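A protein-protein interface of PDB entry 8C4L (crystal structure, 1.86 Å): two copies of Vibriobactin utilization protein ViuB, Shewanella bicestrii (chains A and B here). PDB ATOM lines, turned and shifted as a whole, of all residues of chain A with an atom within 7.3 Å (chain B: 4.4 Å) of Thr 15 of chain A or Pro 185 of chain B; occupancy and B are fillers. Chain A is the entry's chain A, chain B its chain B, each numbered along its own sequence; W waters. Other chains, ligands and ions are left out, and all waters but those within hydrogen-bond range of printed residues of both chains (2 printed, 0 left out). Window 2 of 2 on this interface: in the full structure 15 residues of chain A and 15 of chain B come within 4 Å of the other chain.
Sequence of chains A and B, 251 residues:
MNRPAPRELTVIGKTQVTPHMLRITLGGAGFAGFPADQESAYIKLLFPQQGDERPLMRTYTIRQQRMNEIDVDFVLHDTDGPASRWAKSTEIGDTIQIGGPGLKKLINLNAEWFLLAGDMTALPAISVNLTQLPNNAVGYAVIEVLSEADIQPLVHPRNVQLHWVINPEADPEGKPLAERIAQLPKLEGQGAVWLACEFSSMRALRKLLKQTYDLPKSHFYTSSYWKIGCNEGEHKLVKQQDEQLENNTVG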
ATOM      1  N   GLY A  13     -15.679  21.351  27.312  1.00  0.00           N
ATOM      2  CA  GLY A  13     -17.121  21.470  27.266  1.00  0.00           C
ATOM      3  C   GLY A  13     -17.742  20.234  26.651  1.00  0.00           C
ATOM      4  O   GLY A  13     -17.114  19.569  25.817  1.00  0.00           O
ATOM      5  N   LYS A  14     -18.972  19.907  27.074  1.00  0.00           N
ATOM      6  CA  LYS A  14     -19.745  18.802  26.530  1.00  0.00           C
ATOM      7  C   LYS A  14     -21.184  19.267  26.431  1.00  0.00           C
ATOM      8  O   LYS A  14     -21.712  19.891  27.370  1.00  0.00           O
ATOM      9  CB  LYS A  14     -19.680  17.535  27.411  1.00  0.00           C
ATOM     10  CG  LYS A  14     -18.281  16.987  27.618  1.00  0.00           C
ATOM     11  CD  LYS A  14     -18.297  15.758  28.471  1.00  0.00           C
ATOM     12  CE  LYS A  14     -18.684  14.563  27.633  1.00  0.00           C
ATOM     13  NZ  LYS A  14     -18.560  13.297  28.393  1.00  0.00           N
ATOM     14  N   THR A  15     -21.812  18.916  25.311  1.00  0.00           N
ATOM     15  CA  THR A  15     -23.175  19.313  24.987  1.00  0.00           C
ATOM     16  C   THR A  15     -23.836  18.151  24.279  1.00  0.00           C
ATOM     17  O   THR A  15     -23.367  17.711  23.223  1.00  0.00           O
ATOM     18  CB  THR A  15     -23.221  20.563  24.070  1.00  0.00           C
ATOM     19  OG1 THR A  15     -22.716  21.713  24.771  1.00  0.00           O
ATOM     20  CG2 THR A  15     -24.686  20.886  23.666  1.00  0.00           C
ATOM     21  N   GLN A  16     -24.951  17.711  24.810  1.00  0.00           N
ATOM     22  CA  GLN A  16     -25.774  16.708  24.144  1.00  0.00           C
ATOM     23  C   GLN A  16     -26.586  17.428  23.079  1.00  0.00           C
ATOM     24  O   GLN A  16     -27.542  18.127  23.389  1.00  0.00           O
ATOM     25  CB  GLN A  16     -26.673  16.015  25.157  1.00  0.00           C
ATOM     26  CG  GLN A  16     -27.262  14.723  24.647  1.00  0.00           C
ATOM     27  CD  GLN A  16     -26.237  13.606  24.602  1.00  0.00           C
ATOM     28  OE1 GLN A  16     -25.505  13.376  25.566  1.00  0.00           O
ATOM     29  NE2 GLN A  16     -26.173  12.906  23.476  1.00  0.00           N
ATOM     30  N   VAL A  17     -26.162  17.345  21.824  1.00  0.00           N
ATOM     31  CA  VAL A  17     -26.874  18.061  20.763  1.00  0.00           C
ATOM     32  C   VAL A  17     -28.233  17.421  20.499  1.00  0.00           C
ATOM     33  O   VAL A  17     -29.257  18.106  20.397  1.00  0.00           O
ATOM     34  CB  VAL A  17     -26.019  18.081  19.483  1.00  0.00           C
ATOM     35  CG1 VAL A  17     -26.698  18.879  18.396  1.00  0.00           C
ATOM     36  CG2 VAL A  17     -24.697  18.641  19.794  1.00  0.00           C
ATOM     37  N   THR A  18     -28.249  16.093  20.324  1.00  0.00           N
ATOM     38  CA  THR A  18     -29.468  15.302  20.223  1.00  0.00           C
ATOM     39  C   THR A  18     -29.185  14.015  20.978  1.00  0.00           C
ATOM     40  O   THR A  18     -28.056  13.827  21.451  1.00  0.00           O
ATOM     41  CB  THR A  18     -29.849  15.019  18.769  1.00  0.00           C
ATOM     42  OG1 THR A  18     -28.861  14.172  18.169  1.00  0.00           O
ATOM     43  CG2 THR A  18     -29.948  16.287  17.942  1.00  0.00           C
ATOM     44  N   MET A  21     -26.120  12.380  19.449  1.00  0.00           N
ATOM     45  CA  MET A  21     -25.027  13.224  18.958  1.00  0.00           C
ATOM     46  C   MET A  21     -24.489  14.023  20.134  1.00  0.00           C
ATOM     47  O   MET A  21     -25.219  14.813  20.750  1.00  0.00           O
ATOM     48  CB  MET A  21     -25.451  14.167  17.827  1.00  0.00           C
ATOM     49  CG  MET A  21     -24.213  14.850  17.158  1.00  0.00           C
ATOM     50  SD  MET A  21     -23.265  13.676  16.122  1.00  0.00           S
ATOM     51  CE  MET A  21     -24.092  13.823  14.556  1.00  0.00           C
ATOM     52  N   LEU A  22     -23.239  13.763  20.488  1.00  0.00           N
ATOM     53  CA  LEU A  22     -22.612  14.370  21.658  1.00  0.00           C
ATOM     54  C   LEU A  22     -21.440  15.221  21.193  1.00  0.00           C
ATOM     55  O   LEU A  22     -20.545  14.717  20.519  1.00  0.00           O
ATOM     56  CB  LEU A  22     -22.154  13.287  22.624  1.00  0.00           C
ATOM     57  CG  LEU A  22     -21.347  13.736  23.845  1.00  0.00           C
ATOM     58  CD1 LEU A  22     -22.145  14.698  24.734  1.00  0.00           C
ATOM     59  CD2 LEU A  22     -20.935  12.552  24.640  1.00  0.00           C
ATOM     60  N   ARG A  23     -21.459  16.507  21.519  1.00  0.00           N
ATOM     61  CA  ARG A  23     -20.443  17.447  21.064  1.00  0.00           C
ATOM     62  C   ARG A  23     -19.439  17.697  22.181  1.00  0.00           C
ATOM     63  O   ARG A  23     -19.826  18.079  23.301  1.00  0.00           O
ATOM     64  CB  ARG A  23     -21.108  18.745  20.619  1.00  0.00           C
ATOM     65  CG  ARG A  23     -20.164  19.900  20.348  1.00  0.00           C
ATOM     66  CD  ARG A  23     -20.894  21.062  19.682  1.00  0.00           C
ATOM     67  NE  ARG A  23     -21.533  20.640  18.441  1.00  0.00           N
ATOM     68  CZ  ARG A  23     -22.593  21.219  17.891  1.00  0.00           C
ATOM     69  NH1 ARG A  23     -23.136  22.306  18.415  1.00  0.00           N
ATOM     70  NH2 ARG A  23     -23.149  20.665  16.811  1.00  0.00           N
ATOM     71  N   ILE A  24     -18.159  17.454  21.885  1.00  0.00           N
ATOM     72  CA  ILE A  24     -17.055  17.686  22.806  1.00  0.00           C
ATOM     73  C   ILE A  24     -16.253  18.883  22.306  1.00  0.00           C
ATOM     74  O   ILE A  24     -15.839  18.913  21.139  1.00  0.00           O
ATOM     75  CB  ILE A  24     -16.127  16.467  22.898  1.00  0.00           C
ATOM     76  CG1 ILE A  24     -16.878  15.135  23.115  1.00  0.00           C
ATOM     77  CG2 ILE A  24     -15.119  16.698  23.973  1.00  0.00           C
ATOM     78  CD1 ILE A  24     -17.527  14.982  24.338  1.00  0.00           C
ATOM     79  N   THR A  25     -16.005  19.848  23.186  1.00  0.00           N
ATOM     80  CA  THR A  25     -15.169  20.995  22.868  1.00  0.00           C
ATOM     81  C   THR A  25     -13.747  20.748  23.390  1.00  0.00           C
ATOM     82  O   THR A  25     -13.548  20.341  24.543  1.00  0.00           O
ATOM     83  CB  THR A  25     -15.741  22.277  23.476  1.00  0.00           C
ATOM     84  OG1 THR A  25     -17.083  22.493  23.017  1.00  0.00           O
ATOM     85  CG2 THR A  25     -14.848  23.476  23.083  1.00  0.00           C
ATOM     86  N   GLN A  64     -16.955  22.713  14.391  1.00  0.00           N
ATOM     87  CA  GLN A  64     -16.868  24.159  14.543  1.00  0.00           C
ATOM     88  C   GLN A  64     -15.470  24.487  15.030  1.00  0.00           C
ATOM     89  O   GLN A  64     -14.847  23.693  15.738  1.00  0.00           O
ATOM     90  CB  GLN A  64     -17.907  24.716  15.542  1.00  0.00           C
ATOM     91  CG  GLN A  64     -19.330  24.625  15.003  1.00  0.00           C
ATOM     92  CD  GLN A  64     -20.376  25.171  15.936  1.00  0.00           C
ATOM     93  OE1 GLN A  64     -21.230  25.958  15.540  1.00  0.00           O
ATOM     94  NE2 GLN A  64     -20.340  24.735  17.177  1.00  0.00           N
ATOM     95  N   VAL A  72     -16.079  18.794  18.259  1.00  0.00           N
ATOM     96  CA  VAL A  72     -16.178  17.545  17.541  1.00  0.00           C
ATOM     97  C   VAL A  72     -17.455  16.870  17.983  1.00  0.00           C
ATOM     98  O   VAL A  72     -17.710  16.752  19.183  1.00  0.00           O
ATOM     99  CB  VAL A  72     -14.968  16.641  17.817  1.00  0.00           C
ATOM    100  CG1 VAL A  72     -15.096  15.315  17.016  1.00  0.00           C
ATOM    101  CG2 VAL A  72     -13.668  17.382  17.479  1.00  0.00           C
ATOM    102  N   ASP A  73     -18.255  16.426  17.012  1.00  0.00           N
ATOM    103  CA  ASP A  73     -19.559  15.822  17.254  1.00  0.00           C
ATOM    104  C   ASP A  73     -19.423  14.307  17.086  1.00  0.00           C
ATOM    105  O   ASP A  73     -18.976  13.831  16.026  1.00  0.00           O
ATOM    106  CB  ASP A  73     -20.609  16.371  16.271  1.00  0.00           C
ATOM    107  CG  ASP A  73     -21.058  17.808  16.592  1.00  0.00           C
ATOM    108  OD1 ASP A  73     -20.473  18.434  17.511  1.00  0.00           O
ATOM    109  OD2 ASP A  73     -22.011  18.302  15.910  1.00  0.00           O
ATOM    110  N   TYR B 140     -26.209  27.151  31.196  1.00  0.00           N
ATOM    111  CA  TYR B 140     -24.787  27.178  30.906  1.00  0.00           C
ATOM    112  C   TYR B 140     -24.072  28.085  31.907  1.00  0.00           C
ATOM    113  O   TYR B 140     -24.599  29.127  32.313  1.00  0.00           O
ATOM    114  CB  TYR B 140     -24.468  27.727  29.483  1.00  0.00           C
ATOM    115  CG  TYR B 140     -25.188  27.095  28.329  1.00  0.00           C
ATOM    116  CD1 TYR B 140     -25.055  25.738  28.066  1.00  0.00           C
ATOM    117  CD2 TYR B 140     -25.944  27.852  27.459  1.00  0.00           C
ATOM    118  CE1 TYR B 140     -25.711  25.134  27.006  1.00  0.00           C
ATOM    119  CE2 TYR B 140     -26.604  27.248  26.371  1.00  0.00           C
ATOM    120  CZ  TYR B 140     -26.465  25.887  26.162  1.00  0.00           C
ATOM    121  OH  TYR B 140     -27.066  25.244  25.106  1.00  0.00           O
ATOM    122  N   HIS B 163     -18.711  25.381  30.791  1.00  0.00           N
ATOM    123  CA  HIS B 163     -17.951  25.543  29.565  1.00  0.00           C
ATOM    124  C   HIS B 163     -16.790  26.452  29.876  1.00  0.00           C
ATOM    125  O   HIS B 163     -16.974  27.541  30.433  1.00  0.00           O
ATOM    126  CB  HIS B 163     -18.819  26.112  28.450  1.00  0.00           C
ATOM    127  CG  HIS B 163     -19.799  25.130  27.929  1.00  0.00           C
ATOM    128  ND1 HIS B 163     -19.488  24.234  26.935  1.00  0.00           N
ATOM    129  CD2 HIS B 163     -21.086  24.895  28.264  1.00  0.00           C
ATOM    130  CE1 HIS B 163     -20.535  23.466  26.696  1.00  0.00           C
ATOM    131  NE2 HIS B 163     -21.524  23.856  27.481  1.00  0.00           N
ATOM    132  N   GLN B 183     -22.273  29.830  19.571  1.00  0.00           N
ATOM    133  CA  GLN B 183     -22.178  28.525  18.939  1.00  0.00           C
ATOM    134  C   GLN B 183     -22.652  27.428  19.866  1.00  0.00           C
ATOM    135  O   GLN B 183     -22.335  26.255  19.635  1.00  0.00           O
ATOM    136  CB  GLN B 183     -20.731  28.284  18.474  1.00  0.00           C
ATOM    137  CG  GLN B 183     -20.374  29.266  17.314  1.00  0.00           C
ATOM    138  CD  GLN B 183     -18.962  29.165  16.755  1.00  0.00           C
ATOM    139  OE1 GLN B 183     -18.311  28.125  16.803  1.00  0.00           O
ATOM    140  NE2 GLN B 183     -18.496  30.273  16.179  1.00  0.00           N
ATOM    141  N   LEU B 184     -23.305  27.811  21.000  1.00  0.00           N
ATOM    142  CA  LEU B 184     -24.045  26.910  21.872  1.00  0.00           C
ATOM    143  C   LEU B 184     -25.498  26.885  21.456  1.00  0.00           C
ATOM    144  O   LEU B 184     -26.018  27.892  20.979  1.00  0.00           O
ATOM    145  CB  LEU B 184     -23.965  27.346  23.331  1.00  0.00           C
ATOM    146  CG  LEU B 184     -22.614  27.139  24.032  1.00  0.00           C
ATOM    147  CD1 LEU B 184     -22.604  27.867  25.392  1.00  0.00           C
ATOM    148  CD2 LEU B 184     -22.295  25.645  24.213  1.00  0.00           C
ATOM    149  N   PRO B 185     -26.189  25.756  21.640  1.00  0.00           N
ATOM    150  CA  PRO B 185     -27.622  25.747  21.350  1.00  0.00           C
ATOM    151  C   PRO B 185     -28.345  26.814  22.153  1.00  0.00           C
ATOM    152  O   PRO B 185     -27.950  27.171  23.261  1.00  0.00           O
ATOM    153  CB  PRO B 185     -28.052  24.335  21.736  1.00  0.00           C
ATOM    154  CG  PRO B 185     -26.796  23.499  21.545  1.00  0.00           C
ATOM    155  CD  PRO B 185     -25.689  24.405  21.992  1.00  0.00           C
ATOM    156  N   LYS B 186     -29.379  27.360  21.545  1.00  0.00           N
ATOM    157  CA  LYS B 186     -30.195  28.390  22.168  1.00  0.00           C
ATOM    158  C   LYS B 186     -31.113  27.756  23.204  1.00  0.00           C
ATOM    159  O   LYS B 186     -31.663  26.673  22.992  1.00  0.00           O
ATOM    160  CB  LYS B 186     -31.010  29.123  21.100  1.00  0.00           C
ATOM    161  CG  LYS B 186     -32.022  30.155  21.639  1.00  0.00           C
ATOM    162  CD  LYS B 186     -32.779  30.907  20.518  1.00  0.00           C
ATOM    163  CE  LYS B 186     -33.841  31.884  21.085  1.00  0.00           C
ATOM    164  NZ  LYS B 186     -34.279  32.985  20.129  1.00  0.00           N
ATOM    165  N   LEU B 187     -31.253  28.423  24.341  1.00  0.00           N
ATOM    166  CA  LEU B 187     -32.080  27.914  25.422  1.00  0.00           C
ATOM    167  C   LEU B 187     -33.509  28.375  25.205  1.00  0.00           C
ATOM    168  O   LEU B 187     -33.751  29.489  24.736  1.00  0.00           O
ATOM    169  CB  LEU B 187     -31.555  28.383  26.785  1.00  0.00           C
ATOM    170  CG  LEU B 187     -30.154  27.864  27.121  1.00  0.00           C
ATOM    171  CD1 LEU B 187     -29.605  28.501  28.400  1.00  0.00           C
ATOM    172  CD2 LEU B 187     -30.152  26.335  27.240  1.00  0.00           C
HETATM  173  O   HOH W   1     -23.729  22.068  27.263  1.00  0.00           O
HETATM  174  O   HOH W   2     -22.258  23.940  20.639  1.00  0.00           O
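O of Gly 13 of chain A lies within hydrogen-bond range of N of Thr 25 of chain A, at 2.9 Å. The backbone NH of Arg 23 of chain A lies within hydrogen-bond range of the backbone carbonyl oxygen of Thr 15 of chain A, at 2.8 Å. OH of Tyr 140 of chain B is in hydrogen-bond range of O of Pro 185 of chain B.
ND1 of His 163 of chain B touches CA of Gly 13 of chain A, at 3.7 Å. Lys 14 of chain A touches His 163 of chain B (O to CE1, 3.8 Å). His 163 of chain B touches Thr 15 of chain A. Leu 184 of chain B touches Thr 15 of chain A. CG of Pro 185 of chain B touches CG2 of Thr 15 of chain A, at 3.97 Å. O of Gln 183 of chain B touches NE2 of Gln 64 of chain A, 3.5 Å away.
Of the printed residues of chain B, Gly 13 of chain A touches His 163 (3.7 Å). Printed residues of chain B within 4 Å of Lys 14 of chain A: His 163 (3.8 Å). Of the printed residues of chain B, Thr 15 of chain A touches His 163, Leu 184 and Pro 185. Of the printed residues of chain B, Gln 64 of chain A touches Gln 183 (3.5 Å). Of the printed residues of chain A, His 163 of chain B touches Gly 13, Lys 14 and Thr 15. Of the printed residues of chain A, Gln 183 of chain B touches Gln 64. Pro 185 of chain B touches just one residue of chain A: Thr 15 (3.97 Å). The nearest printed residue of chain B that does not touch Thr 15 of chain A is Tyr 140 of chain B (5.1 Å).
Of the 7 printed residues of chain B, 4 touch a printed residue of chain A. Printed residues of chain B that touch a printed residue of chain A: His 163, Gln 183, Leu 184 and Pro 185.
No position is printed for both chains.
Water W2 lies within hydrogen-bond range of the backbone carbonyl oxygen of Gln 183 of chain B (2.5 Å) and the guanidinium group of Arg 23 of chain A (2.9 Å). Water W1 lies within hydrogen-bond range of the side-chain hydroxyl (OG1) of Thr 15 of chain A, a ring nitrogen (NE2) of His 163 of chain B and the backbone carbonyl oxygen (O) of Lys 14 of chain A.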
